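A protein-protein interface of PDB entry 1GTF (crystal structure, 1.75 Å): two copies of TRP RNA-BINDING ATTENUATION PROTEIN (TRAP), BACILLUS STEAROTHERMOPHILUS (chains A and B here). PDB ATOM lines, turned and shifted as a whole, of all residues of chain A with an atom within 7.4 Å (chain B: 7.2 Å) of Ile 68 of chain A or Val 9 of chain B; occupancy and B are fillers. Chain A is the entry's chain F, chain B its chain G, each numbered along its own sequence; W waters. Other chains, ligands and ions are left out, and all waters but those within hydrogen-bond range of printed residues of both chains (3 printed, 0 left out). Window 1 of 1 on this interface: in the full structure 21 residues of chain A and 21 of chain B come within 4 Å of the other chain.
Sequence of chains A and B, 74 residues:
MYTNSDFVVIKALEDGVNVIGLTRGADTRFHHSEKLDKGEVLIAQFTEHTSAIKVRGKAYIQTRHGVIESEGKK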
ATOM      1  N   VAL A   8     -11.481  27.880  -7.608  1.00  0.00           N
ATOM      2  CA  VAL A   8     -12.900  28.002  -7.310  1.00  0.00           C
ATOM      3  C   VAL A   8     -13.005  28.626  -5.928  1.00  0.00           C
ATOM      4  O   VAL A   8     -12.117  28.419  -5.059  1.00  0.00           O
ATOM      5  CB  VAL A   8     -13.598  26.616  -7.289  1.00  0.00           C
ATOM      6  CG1 VAL A   8     -13.166  25.704  -8.442  1.00  0.00           C
ATOM      7  CG2 VAL A   8     -13.270  25.962  -6.080  1.00  0.00           C
ATOM      8  N   VAL A   9     -14.076  29.381  -5.684  1.00  0.00           N
ATOM      9  CA  VAL A   9     -14.302  29.937  -4.361  1.00  0.00           C
ATOM     10  C   VAL A   9     -15.503  29.178  -3.778  1.00  0.00           C
ATOM     11  O   VAL A   9     -16.531  29.057  -4.428  1.00  0.00           O
ATOM     12  CB  VAL A   9     -14.630  31.438  -4.495  1.00  0.00           C
ATOM     13  CG1 VAL A   9     -15.017  32.089  -3.116  1.00  0.00           C
ATOM     14  CG2 VAL A   9     -13.472  32.221  -5.262  1.00  0.00           C
ATOM     15  N   ALA A  59     -23.551  25.164  -0.066  1.00  0.00           N
ATOM     16  CA  ALA A  59     -22.493  26.131  -0.286  1.00  0.00           C
ATOM     17  C   ALA A  59     -22.766  27.076  -1.445  1.00  0.00           C
ATOM     18  O   ALA A  59     -23.499  26.742  -2.370  1.00  0.00           O
ATOM     19  CB  ALA A  59     -21.163  25.389  -0.538  1.00  0.00           C
ATOM     20  N   TYR A  60     -22.163  28.251  -1.382  1.00  0.00           N
ATOM     21  CA  TYR A  60     -22.232  29.206  -2.503  1.00  0.00           C
ATOM     22  C   TYR A  60     -20.897  29.125  -3.212  1.00  0.00           C
ATOM     23  O   TYR A  60     -19.857  29.264  -2.575  1.00  0.00           O
ATOM     24  CB  TYR A  60     -22.444  30.599  -1.926  1.00  0.00           C
ATOM     25  CG  TYR A  60     -22.818  31.697  -2.916  1.00  0.00           C
ATOM     26  CD1 TYR A  60     -24.155  31.882  -3.305  1.00  0.00           C
ATOM     27  CD2 TYR A  60     -21.877  32.602  -3.361  1.00  0.00           C
ATOM     28  CE1 TYR A  60     -24.523  32.907  -4.173  1.00  0.00           C
ATOM     29  CE2 TYR A  60     -22.241  33.669  -4.278  1.00  0.00           C
ATOM     30  CZ  TYR A  60     -23.564  33.814  -4.651  1.00  0.00           C
ATOM     31  OH  TYR A  60     -23.956  34.859  -5.513  1.00  0.00           O
ATOM     32  N   ILE A  61     -20.894  28.913  -4.530  1.00  0.00           N
ATOM     33  CA  ILE A  61     -19.657  28.596  -5.248  1.00  0.00           C
ATOM     34  C   ILE A  61     -19.523  29.584  -6.401  1.00  0.00           C
ATOM     35  O   ILE A  61     -20.491  29.878  -7.108  1.00  0.00           O
ATOM     36  CB  ILE A  61     -19.687  27.146  -5.808  1.00  0.00           C
ATOM     37  CG1 ILE A  61     -19.805  26.117  -4.659  1.00  0.00           C
ATOM     38  CG2 ILE A  61     -18.421  26.874  -6.706  1.00  0.00           C
ATOM     39  CD1 ILE A  61     -20.503  24.799  -5.040  1.00  0.00           C
ATOM     40  N   GLN A  62     -18.333  30.124  -6.543  1.00  0.00           N
ATOM     41  CA  GLN A  62     -17.995  30.980  -7.709  1.00  0.00           C
ATOM     42  C   GLN A  62     -16.849  30.374  -8.515  1.00  0.00           C
ATOM     43  O   GLN A  62     -15.826  29.929  -7.939  1.00  0.00           O
ATOM     44  CB  GLN A  62     -17.530  32.368  -7.235  1.00  0.00           C
ATOM     45  CG  GLN A  62     -18.537  33.225  -6.542  1.00  0.00           C
ATOM     46  CD  GLN A  62     -17.877  34.380  -5.795  1.00  0.00           C
ATOM     47  OE1 GLN A  62     -16.720  34.273  -5.354  1.00  0.00           O
ATOM     48  NE2 GLN A  62     -18.576  35.495  -5.699  1.00  0.00           N
ATOM     49  N   THR A  63     -17.011  30.303  -9.844  1.00  0.00           N
ATOM     50  CA  THR A  63     -15.904  29.931 -10.730  1.00  0.00           C
ATOM     51  C   THR A  63     -15.889  30.927 -11.872  1.00  0.00           C
ATOM     52  O   THR A  63     -16.744  31.834 -11.914  1.00  0.00           O
ATOM     53  CB  THR A  63     -16.078  28.503 -11.309  1.00  0.00           C
ATOM     54  OG1 THR A  63     -17.082  28.569 -12.312  1.00  0.00           O
ATOM     55  CG2 THR A  63     -16.568  27.502 -10.249  1.00  0.00           C
ATOM     56  N   ARG A  64     -14.954  30.760 -12.823  1.00  0.00           N
ATOM     57  CA  ARG A  64     -14.898  31.604 -14.018  1.00  0.00           C
ATOM     58  C   ARG A  64     -16.207  31.580 -14.800  1.00  0.00           C
ATOM     59  O   ARG A  64     -16.506  32.517 -15.568  1.00  0.00           O
ATOM     60  CB  ARG A  64     -13.745  31.187 -14.944  1.00  0.00           C
ATOM     61  CG  ARG A  64     -13.446  32.155 -16.052  1.00  0.00           C
ATOM     62  CD  ARG A  64     -12.036  32.047 -16.584  1.00  0.00           C
ATOM     63  NE  ARG A  64     -11.813  30.741 -17.206  1.00  0.00           N
ATOM     64  N   HIS A  65     -16.988  30.506 -14.617  1.00  0.00           N
ATOM     65  CA  HIS A  65     -18.239  30.355 -15.377  1.00  0.00           C
ATOM     66  C   HIS A  65     -19.456  30.969 -14.665  1.00  0.00           C
ATOM     67  O   HIS A  65     -20.545  31.016 -15.243  1.00  0.00           O
ATOM     68  CB  HIS A  65     -18.521  28.888 -15.740  1.00  0.00           C
ATOM     69  CG  HIS A  65     -17.381  28.190 -16.414  1.00  0.00           C
ATOM     70  ND1 HIS A  65     -16.543  28.821 -17.309  1.00  0.00           N
ATOM     71  CD2 HIS A  65     -16.991  26.891 -16.382  1.00  0.00           C
ATOM     72  CE1 HIS A  65     -15.627  27.961 -17.725  1.00  0.00           C
ATOM     73  NE2 HIS A  65     -15.899  26.776 -17.197  1.00  0.00           N
ATOM     74  N   GLY A  66     -19.259  31.478 -13.460  1.00  0.00           N
ATOM     75  CA  GLY A  66     -20.317  32.190 -12.741  1.00  0.00           C
ATOM     76  C   GLY A  66     -20.625  31.492 -11.435  1.00  0.00           C
ATOM     77  O   GLY A  66     -19.800  30.787 -10.880  1.00  0.00           O
ATOM     78  N   VAL A  67     -21.834  31.688 -10.935  1.00  0.00           N
ATOM     79  CA  VAL A  67     -22.171  31.202  -9.606  1.00  0.00           C
ATOM     80  C   VAL A  67     -22.958  29.917  -9.728  1.00  0.00           C
ATOM     81  O   VAL A  67     -23.734  29.754 -10.678  1.00  0.00           O
ATOM     82  CB  VAL A  67     -23.034  32.289  -8.895  1.00  0.00           C
ATOM     83  CG1 VAL A  67     -23.598  31.811  -7.593  1.00  0.00           C
ATOM     84  CG2 VAL A  67     -22.185  33.577  -8.698  1.00  0.00           C
ATOM     85  N   ILE A  68     -22.791  29.009  -8.763  1.00  0.00           N
ATOM     86  CA  ILE A  68     -23.637  27.801  -8.705  1.00  0.00           C
ATOM     87  C   ILE A  68     -23.757  27.546  -7.204  1.00  0.00           C
ATOM     88  O   ILE A  68     -22.916  27.993  -6.429  1.00  0.00           O
ATOM     89  CB  ILE A  68     -22.998  26.593  -9.447  1.00  0.00           C
ATOM     90  CG1 ILE A  68     -23.981  25.408  -9.566  1.00  0.00           C
ATOM     91  CG2 ILE A  68     -21.679  26.154  -8.784  1.00  0.00           C
ATOM     92  CD1 ILE A  68     -24.492  25.139 -10.954  1.00  0.00           C
ATOM     93  N   GLU A  69     -24.811  26.872  -6.781  1.00  0.00           N
ATOM     94  CA  GLU A  69     -24.919  26.585  -5.370  1.00  0.00           C
ATOM     95  C   GLU A  69     -25.125  25.094  -5.186  1.00  0.00           C
ATOM     96  O   GLU A  69     -25.937  24.483  -5.877  1.00  0.00           O
ATOM     97  CB  GLU A  69     -26.086  27.365  -4.740  1.00  0.00           C
ATOM     98  N   SER A  70     -24.360  24.497  -4.283  1.00  0.00           N
ATOM     99  CA  SER A  70     -24.645  23.104  -3.928  1.00  0.00           C
ATOM    100  C   SER A  70     -25.667  23.094  -2.803  1.00  0.00           C
ATOM    101  O   SER A  70     -25.799  24.055  -2.038  1.00  0.00           O
ATOM    102  CB  SER A  70     -23.367  22.372  -3.502  1.00  0.00           C
ATOM    103  OG  SER A  70     -22.727  23.089  -2.455  1.00  0.00           O
ATOM    104  N   PHE B   7     -12.457  23.617 -17.686  1.00  0.00           N
ATOM    105  CA  PHE B   7     -13.178  22.739 -16.756  1.00  0.00           C
ATOM    106  C   PHE B   7     -14.684  22.852 -16.964  1.00  0.00           C
ATOM    107  O   PHE B   7     -15.163  23.795 -17.551  1.00  0.00           O
ATOM    108  CB  PHE B   7     -12.788  23.092 -15.296  1.00  0.00           C
ATOM    109  CG  PHE B   7     -13.205  24.491 -14.867  1.00  0.00           C
ATOM    110  CD1 PHE B   7     -14.483  24.717 -14.336  1.00  0.00           C
ATOM    111  CD2 PHE B   7     -12.382  25.582 -15.077  1.00  0.00           C
ATOM    112  CE1 PHE B   7     -14.863  26.024 -13.936  1.00  0.00           C
ATOM    113  CE2 PHE B   7     -12.764  26.875 -14.711  1.00  0.00           C
ATOM    114  CZ  PHE B   7     -14.009  27.104 -14.145  1.00  0.00           C
ATOM    115  N   VAL B   8     -15.455  21.911 -16.446  1.00  0.00           N
ATOM    116  CA  VAL B   8     -16.896  21.993 -16.602  1.00  0.00           C
ATOM    117  C   VAL B   8     -17.415  21.939 -15.181  1.00  0.00           C
ATOM    118  O   VAL B   8     -16.788  21.274 -14.333  1.00  0.00           O
ATOM    119  CB  VAL B   8     -17.445  20.744 -17.349  1.00  0.00           C
ATOM    120  CG1 VAL B   8     -16.836  20.593 -18.707  1.00  0.00           C
ATOM    121  CG2 VAL B   8     -17.020  19.519 -16.680  1.00  0.00           C
ATOM    122  N   VAL B   9     -18.558  22.592 -14.913  1.00  0.00           N
ATOM    123  CA  VAL B   9     -19.207  22.511 -13.605  1.00  0.00           C
ATOM    124  C   VAL B   9     -20.466  21.703 -13.844  1.00  0.00           C
ATOM    125  O   VAL B   9     -21.219  21.976 -14.777  1.00  0.00           O
ATOM    126  CB  VAL B   9     -19.576  23.927 -13.093  1.00  0.00           C
ATOM    127  CG1 VAL B   9     -20.379  23.872 -11.739  1.00  0.00           C
ATOM    128  CG2 VAL B   9     -18.303  24.810 -12.966  1.00  0.00           C
ATOM    129  N   ILE B  10     -20.686  20.712 -12.990  1.00  0.00           N
ATOM    130  CA  ILE B  10     -21.896  19.896 -13.023  1.00  0.00           C
ATOM    131  C   ILE B  10     -22.614  19.871 -11.666  1.00  0.00           C
ATOM    132  O   ILE B  10     -22.049  19.465 -10.657  1.00  0.00           O
ATOM    133  CB  ILE B  10     -21.575  18.431 -13.499  1.00  0.00           C
ATOM    134  CG1 ILE B  10     -20.843  18.537 -14.847  1.00  0.00           C
ATOM    135  CG2 ILE B  10     -22.873  17.600 -13.594  1.00  0.00           C
ATOM    136  CD1 ILE B  10     -19.495  17.929 -14.793  1.00  0.00           C
ATOM    137  N   LYS B  11     -23.883  20.276 -11.643  1.00  0.00           N
ATOM    138  CA  LYS B  11     -24.663  20.184 -10.429  1.00  0.00           C
ATOM    139  C   LYS B  11     -25.755  19.139 -10.653  1.00  0.00           C
ATOM    140  O   LYS B  11     -26.546  19.285 -11.566  1.00  0.00           O
ATOM    141  CB  LYS B  11     -25.333  21.531 -10.136  1.00  0.00           C
ATOM    142  CG  LYS B  11     -26.198  21.470  -8.879  1.00  0.00           C
ATOM    143  CD  LYS B  11     -26.995  22.758  -8.662  1.00  0.00           C
ATOM    144  CE  LYS B  11     -27.859  22.648  -7.400  1.00  0.00           C
ATOM    145  NZ  LYS B  11     -28.483  23.985  -7.095  1.00  0.00           N
ATOM    146  N   VAL B  41     -22.107  19.182  -6.283  1.00  0.00           N
ATOM    147  CA  VAL B  41     -21.468  19.837  -7.440  1.00  0.00           C
ATOM    148  C   VAL B  41     -20.100  19.243  -7.703  1.00  0.00           C
ATOM    149  O   VAL B  41     -19.326  19.038  -6.769  1.00  0.00           O
ATOM    150  CB  VAL B  41     -21.285  21.371  -7.148  1.00  0.00           C
ATOM    151  CG1 VAL B  41     -20.496  22.003  -8.247  1.00  0.00           C
ATOM    152  CG2 VAL B  41     -22.634  22.043  -6.948  1.00  0.00           C
ATOM    153  N   LEU B  42     -19.772  19.047  -8.979  1.00  0.00           N
ATOM    154  CA  LEU B  42     -18.441  18.558  -9.374  1.00  0.00           C
ATOM    155  C   LEU B  42     -17.883  19.556 -10.339  1.00  0.00           C
ATOM    156  O   LEU B  42     -18.583  19.987 -11.245  1.00  0.00           O
ATOM    157  CB  LEU B  42     -18.540  17.229 -10.107  1.00  0.00           C
ATOM    158  CG  LEU B  42     -17.205  16.564 -10.507  1.00  0.00           C
ATOM    159  CD1 LEU B  42     -16.480  16.097  -9.219  1.00  0.00           C
ATOM    160  CD2 LEU B  42     -17.576  15.337 -11.385  1.00  0.00           C
ATOM    161  N   ILE B  43     -16.645  19.958 -10.110  1.00  0.00           N
ATOM    162  CA  ILE B  43     -15.956  20.863 -11.059  1.00  0.00           C
ATOM    163  C   ILE B  43     -14.743  20.040 -11.571  1.00  0.00           C
ATOM    164  O   ILE B  43     -13.841  19.713 -10.798  1.00  0.00           O
ATOM    165  CB  ILE B  43     -15.484  22.094 -10.323  1.00  0.00           C
ATOM    166  CG1 ILE B  43     -16.671  22.745  -9.567  1.00  0.00           C
ATOM    167  CG2 ILE B  43     -14.880  23.053 -11.381  1.00  0.00           C
ATOM    168  CD1 ILE B  43     -16.508  22.900  -8.088  1.00  0.00           C
ATOM    169  N   ALA B  44     -14.720  19.743 -12.866  1.00  0.00           N
ATOM    170  CA  ALA B  44     -13.810  18.717 -13.403  1.00  0.00           C
ATOM    171  C   ALA B  44     -13.103  19.273 -14.616  1.00  0.00           C
ATOM    172  O   ALA B  44     -13.752  19.810 -15.503  1.00  0.00           O
ATOM    173  CB  ALA B  44     -14.568  17.521 -13.791  1.00  0.00           C
ATOM    174  N   VAL B  55     -22.174  13.302 -19.470  1.00  0.00           N
ATOM    175  CA  VAL B  55     -23.026  13.451 -18.288  1.00  0.00           C
ATOM    176  C   VAL B  55     -24.316  12.711 -18.572  1.00  0.00           C
ATOM    177  O   VAL B  55     -24.940  12.915 -19.621  1.00  0.00           O
ATOM    178  CB  VAL B  55     -23.309  14.922 -17.933  1.00  0.00           C
ATOM    179  CG1 VAL B  55     -24.064  15.002 -16.616  1.00  0.00           C
ATOM    180  CG2 VAL B  55     -21.954  15.729 -17.835  1.00  0.00           C
ATOM    181  N   ALA B  59     -28.993  17.135 -14.867  1.00  0.00           N
ATOM    182  CA  ALA B  59     -28.035  18.016 -14.230  1.00  0.00           C
ATOM    183  C   ALA B  59     -27.967  19.395 -14.876  1.00  0.00           C
ATOM    184  O   ALA B  59     -28.319  19.583 -16.045  1.00  0.00           O
ATOM    185  CB  ALA B  59     -26.669  17.370 -14.278  1.00  0.00           C
ATOM    186  N   TYR B  60     -27.462  20.333 -14.104  1.00  0.00           N
ATOM    187  CA  TYR B  60     -27.208  21.701 -14.608  1.00  0.00           C
ATOM    188  C   TYR B  60     -25.708  21.797 -14.865  1.00  0.00           C
ATOM    189  O   TYR B  60     -24.896  21.531 -13.966  1.00  0.00           O
ATOM    190  CB  TYR B  60     -27.657  22.663 -13.510  1.00  0.00           C
ATOM    191  CG  TYR B  60     -27.863  24.100 -13.939  1.00  0.00           C
ATOM    192  CD1 TYR B  60     -29.070  24.504 -14.492  1.00  0.00           C
ATOM    193  CD2 TYR B  60     -26.897  25.039 -13.720  1.00  0.00           C
ATOM    194  CE1 TYR B  60     -29.294  25.833 -14.861  1.00  0.00           C
ATOM    195  CE2 TYR B  60     -27.088  26.393 -14.119  1.00  0.00           C
ATOM    196  CZ  TYR B  60     -28.291  26.773 -14.657  1.00  0.00           C
ATOM    197  OH  TYR B  60     -28.524  28.091 -15.030  1.00  0.00           O
ATOM    198  N   ILE B  61     -25.314  22.221 -16.066  1.00  0.00           N
ATOM    199  CA  ILE B  61     -23.916  22.177 -16.448  1.00  0.00           C
ATOM    200  C   ILE B  61     -23.461  23.561 -16.932  1.00  0.00           C
ATOM    201  O   ILE B  61     -24.173  24.201 -17.689  1.00  0.00           O
ATOM    202  CB  ILE B  61     -23.690  21.132 -17.609  1.00  0.00           C
ATOM    203  CG1 ILE B  61     -24.056  19.695 -17.211  1.00  0.00           C
ATOM    204  CG2 ILE B  61     -22.226  21.204 -18.123  1.00  0.00           C
ATOM    205  CD1 ILE B  61     -24.501  18.780 -18.418  1.00  0.00           C
ATOM    206  N   GLN B  62     -22.310  24.031 -16.480  1.00  0.00           N
ATOM    207  CA  GLN B  62     -21.750  25.300 -16.995  1.00  0.00           C
ATOM    208  C   GLN B  62     -20.399  25.028 -17.603  1.00  0.00           C
ATOM    209  O   GLN B  62     -19.570  24.316 -16.988  1.00  0.00           O
ATOM    210  CB  GLN B  62     -21.510  26.287 -15.860  1.00  0.00           C
ATOM    211  CG  GLN B  62     -22.768  26.679 -15.076  1.00  0.00           C
ATOM    212  CD  GLN B  62     -22.468  27.389 -13.770  1.00  0.00           C
ATOM    213  OE1 GLN B  62     -21.509  27.053 -13.058  1.00  0.00           O
ATOM    214  NE2 GLN B  62     -23.305  28.360 -13.433  1.00  0.00           N
ATOM    215  N   THR B  63     -20.144  25.651 -18.763  1.00  0.00           N
ATOM    216  CA  THR B  63     -18.836  25.585 -19.392  1.00  0.00           C
ATOM    217  C   THR B  63     -18.574  27.006 -19.876  1.00  0.00           C
ATOM    218  O   THR B  63     -19.422  27.907 -19.719  1.00  0.00           O
ATOM    219  CB  THR B  63     -18.750  24.619 -20.628  1.00  0.00           C
ATOM    220  OG1 THR B  63     -19.427  25.179 -21.765  1.00  0.00           O
ATOM    221  CG2 THR B  63     -19.410  23.299 -20.343  1.00  0.00           C
ATOM    222  N   ILE B  68     -25.941  24.457 -20.099  1.00  0.00           N
ATOM    223  CA  ILE B  68     -26.716  23.446 -20.833  1.00  0.00           C
ATOM    224  C   ILE B  68     -27.232  22.538 -19.745  1.00  0.00           C
ATOM    225  O   ILE B  68     -26.630  22.480 -18.664  1.00  0.00           O
ATOM    226  CB  ILE B  68     -25.867  22.672 -21.850  1.00  0.00           C
ATOM    227  CG1 ILE B  68     -26.772  21.936 -22.861  1.00  0.00           C
ATOM    228  CG2 ILE B  68     -24.874  21.750 -21.132  1.00  0.00           C
ATOM    229  CD1 ILE B  68     -26.329  22.025 -24.292  1.00  0.00           C
HETATM  230  O   HOH W   1     -19.670  28.076 -11.463  1.00  0.00           O
HETATM  231  O   HOH W   2     -15.232  25.344 -20.005  1.00  0.00           O
HETATM  232  O   HOH W   3     -27.465  26.707  -7.993  1.00  0.00           O
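Among the printed residues, merely in contact across the chains: Ser 70 of chain A with Val 41 of chain B (3.5 Å), Ile 68 of chain A with Tyr 60 of chain B (3.7 Å), His 65 of chain A with Gln 62 of chain B (3.7 Å), His 65 of chain A with Thr 63 of chain B (3.7 Å), Thr 63 of chain A with Phe 7 of chain B (3.7 Å), Ile 68 of chain A with Lys 11 of chain B (3.8 Å), Ile 68 of chain A with Gln 62 of chain B (3.9 Å), Ile 68 of chain A with Val 9 of chain B (3.95 Å) and Ile 61 of chain A with Val 41 of chain B (3.97 Å).
Of chain B, only Val 9 (3.95 Å), Lys 11 (3.8 Å), Tyr 60 (3.7 Å) and Gln 62 (3.9 Å) come within 4 Å of Ile 68 of chain A.
Of the printed residues of chain A, Val 9 of chain B touches Ile 68.
Of the printed residues of chain A, Gln 62 of chain B touches His 65 (3.7 Å), Val 67 (3.1 Å) and Ile 68 (3.9 Å).
Of the printed residues of chain A, Val 41 of chain B touches Ile 61 (3.97 Å) and Ser 70 (3.5 Å).
Val 9 of chain A touches none of the printed residues of chain B.
The nearest printed residue of chain B that does not touch Glu 69 of chain A is Val 41 of chain B (4.2 Å).
Water W1 lies within hydrogen-bond range of the side-chain amide oxygen (OE1) of Gln 62 of chain B (2.6 Å), the side-chain hydroxyl (OG1) of Thr 63 of chain A (2.8 Å) and the backbone carbonyl oxygen (O) of Gly 66 of chain A (2.8 Å).
Water W2 bridges the backbone carbonyl oxygen of Phe 7 of chain B (2.9 Å) and a ring nitrogen (NE2) of His 65 of chain A (3.2 Å).
Water W3 lies within hydrogen-bond range of the backbone NH of Glu 69 of chain A (2.9 Å) and the side-chain amino group of Lys 11 of chain B (3.0 Å).
Printed residues of chain B that touch a printed residue of chain A: Phe 7, Val 9, Lys 11, Val 41, Tyr 60, Gln 62 and Thr 63.
Hydrophobic or aromatic side chains of chain B within 4 Å of the printed part of chain A: Phe 7, Val 9, Val 41 and Tyr 60.
Hydrophobic or aromatic side chains of chain A that line the printed part of chain B: Ile 61, His 65 and Ile 68.
Among the printed residues, 12 pairs touch across the chains.
Ile 68 of chain A touches Val 9 of chain B, but with the chains exchanged Val 9 of chain A does not touch Ile 68 of chain B (18.7 Å).
Ile 68 of chain A touches Tyr 60 of chain B, but with the chains exchanged Tyr 60 of chain A does not touch Ile 68 of chain B (17.8 Å).
Ile 68 of chain A touches Gln 62 of chain B, but with the chains exchanged Gln 62 of chain A does not touch Ile 68 of chain B (15.9 Å).
NE2 of His 65 of chain A sits at hydrogen-bond distance from O of Phe 7 of chain B (3.1 Å).
The backbone carbonyl oxygen (O) of Val 67 of chain A is in hydrogen-bond range of the side-chain amide nitrogen (NE2) of Gln 62 of chain B.
The backbone carbonyl oxygen (O) of Glu 69 of chain A sits at hydrogen-bond distance from the side-chain amino group (NZ) of Lys 11 of chain B.
The backbone carbonyl oxygen (O) of Ala 59 of chain A is in hydrogen-bond range of the backbone NH (N) of Ser 70 of chain A (3.1 Å).
O of Ile 68 of chain A sits at hydrogen-bond distance from N of Ile 61 of chain A (2.9 Å).
The backbone NH (N) of His 65 of chain A lies close to the side-chain hydroxyl (OG1) of Thr 63 of chain A (3.0 Å).
N of Val 9 of chain B lies within hydrogen-bond range of O of Gln 62 of chain B, at 2.9 Å.
O of Tyr 60 of chain B sits at hydrogen-bond distance from N of Lys 11 of chain B.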
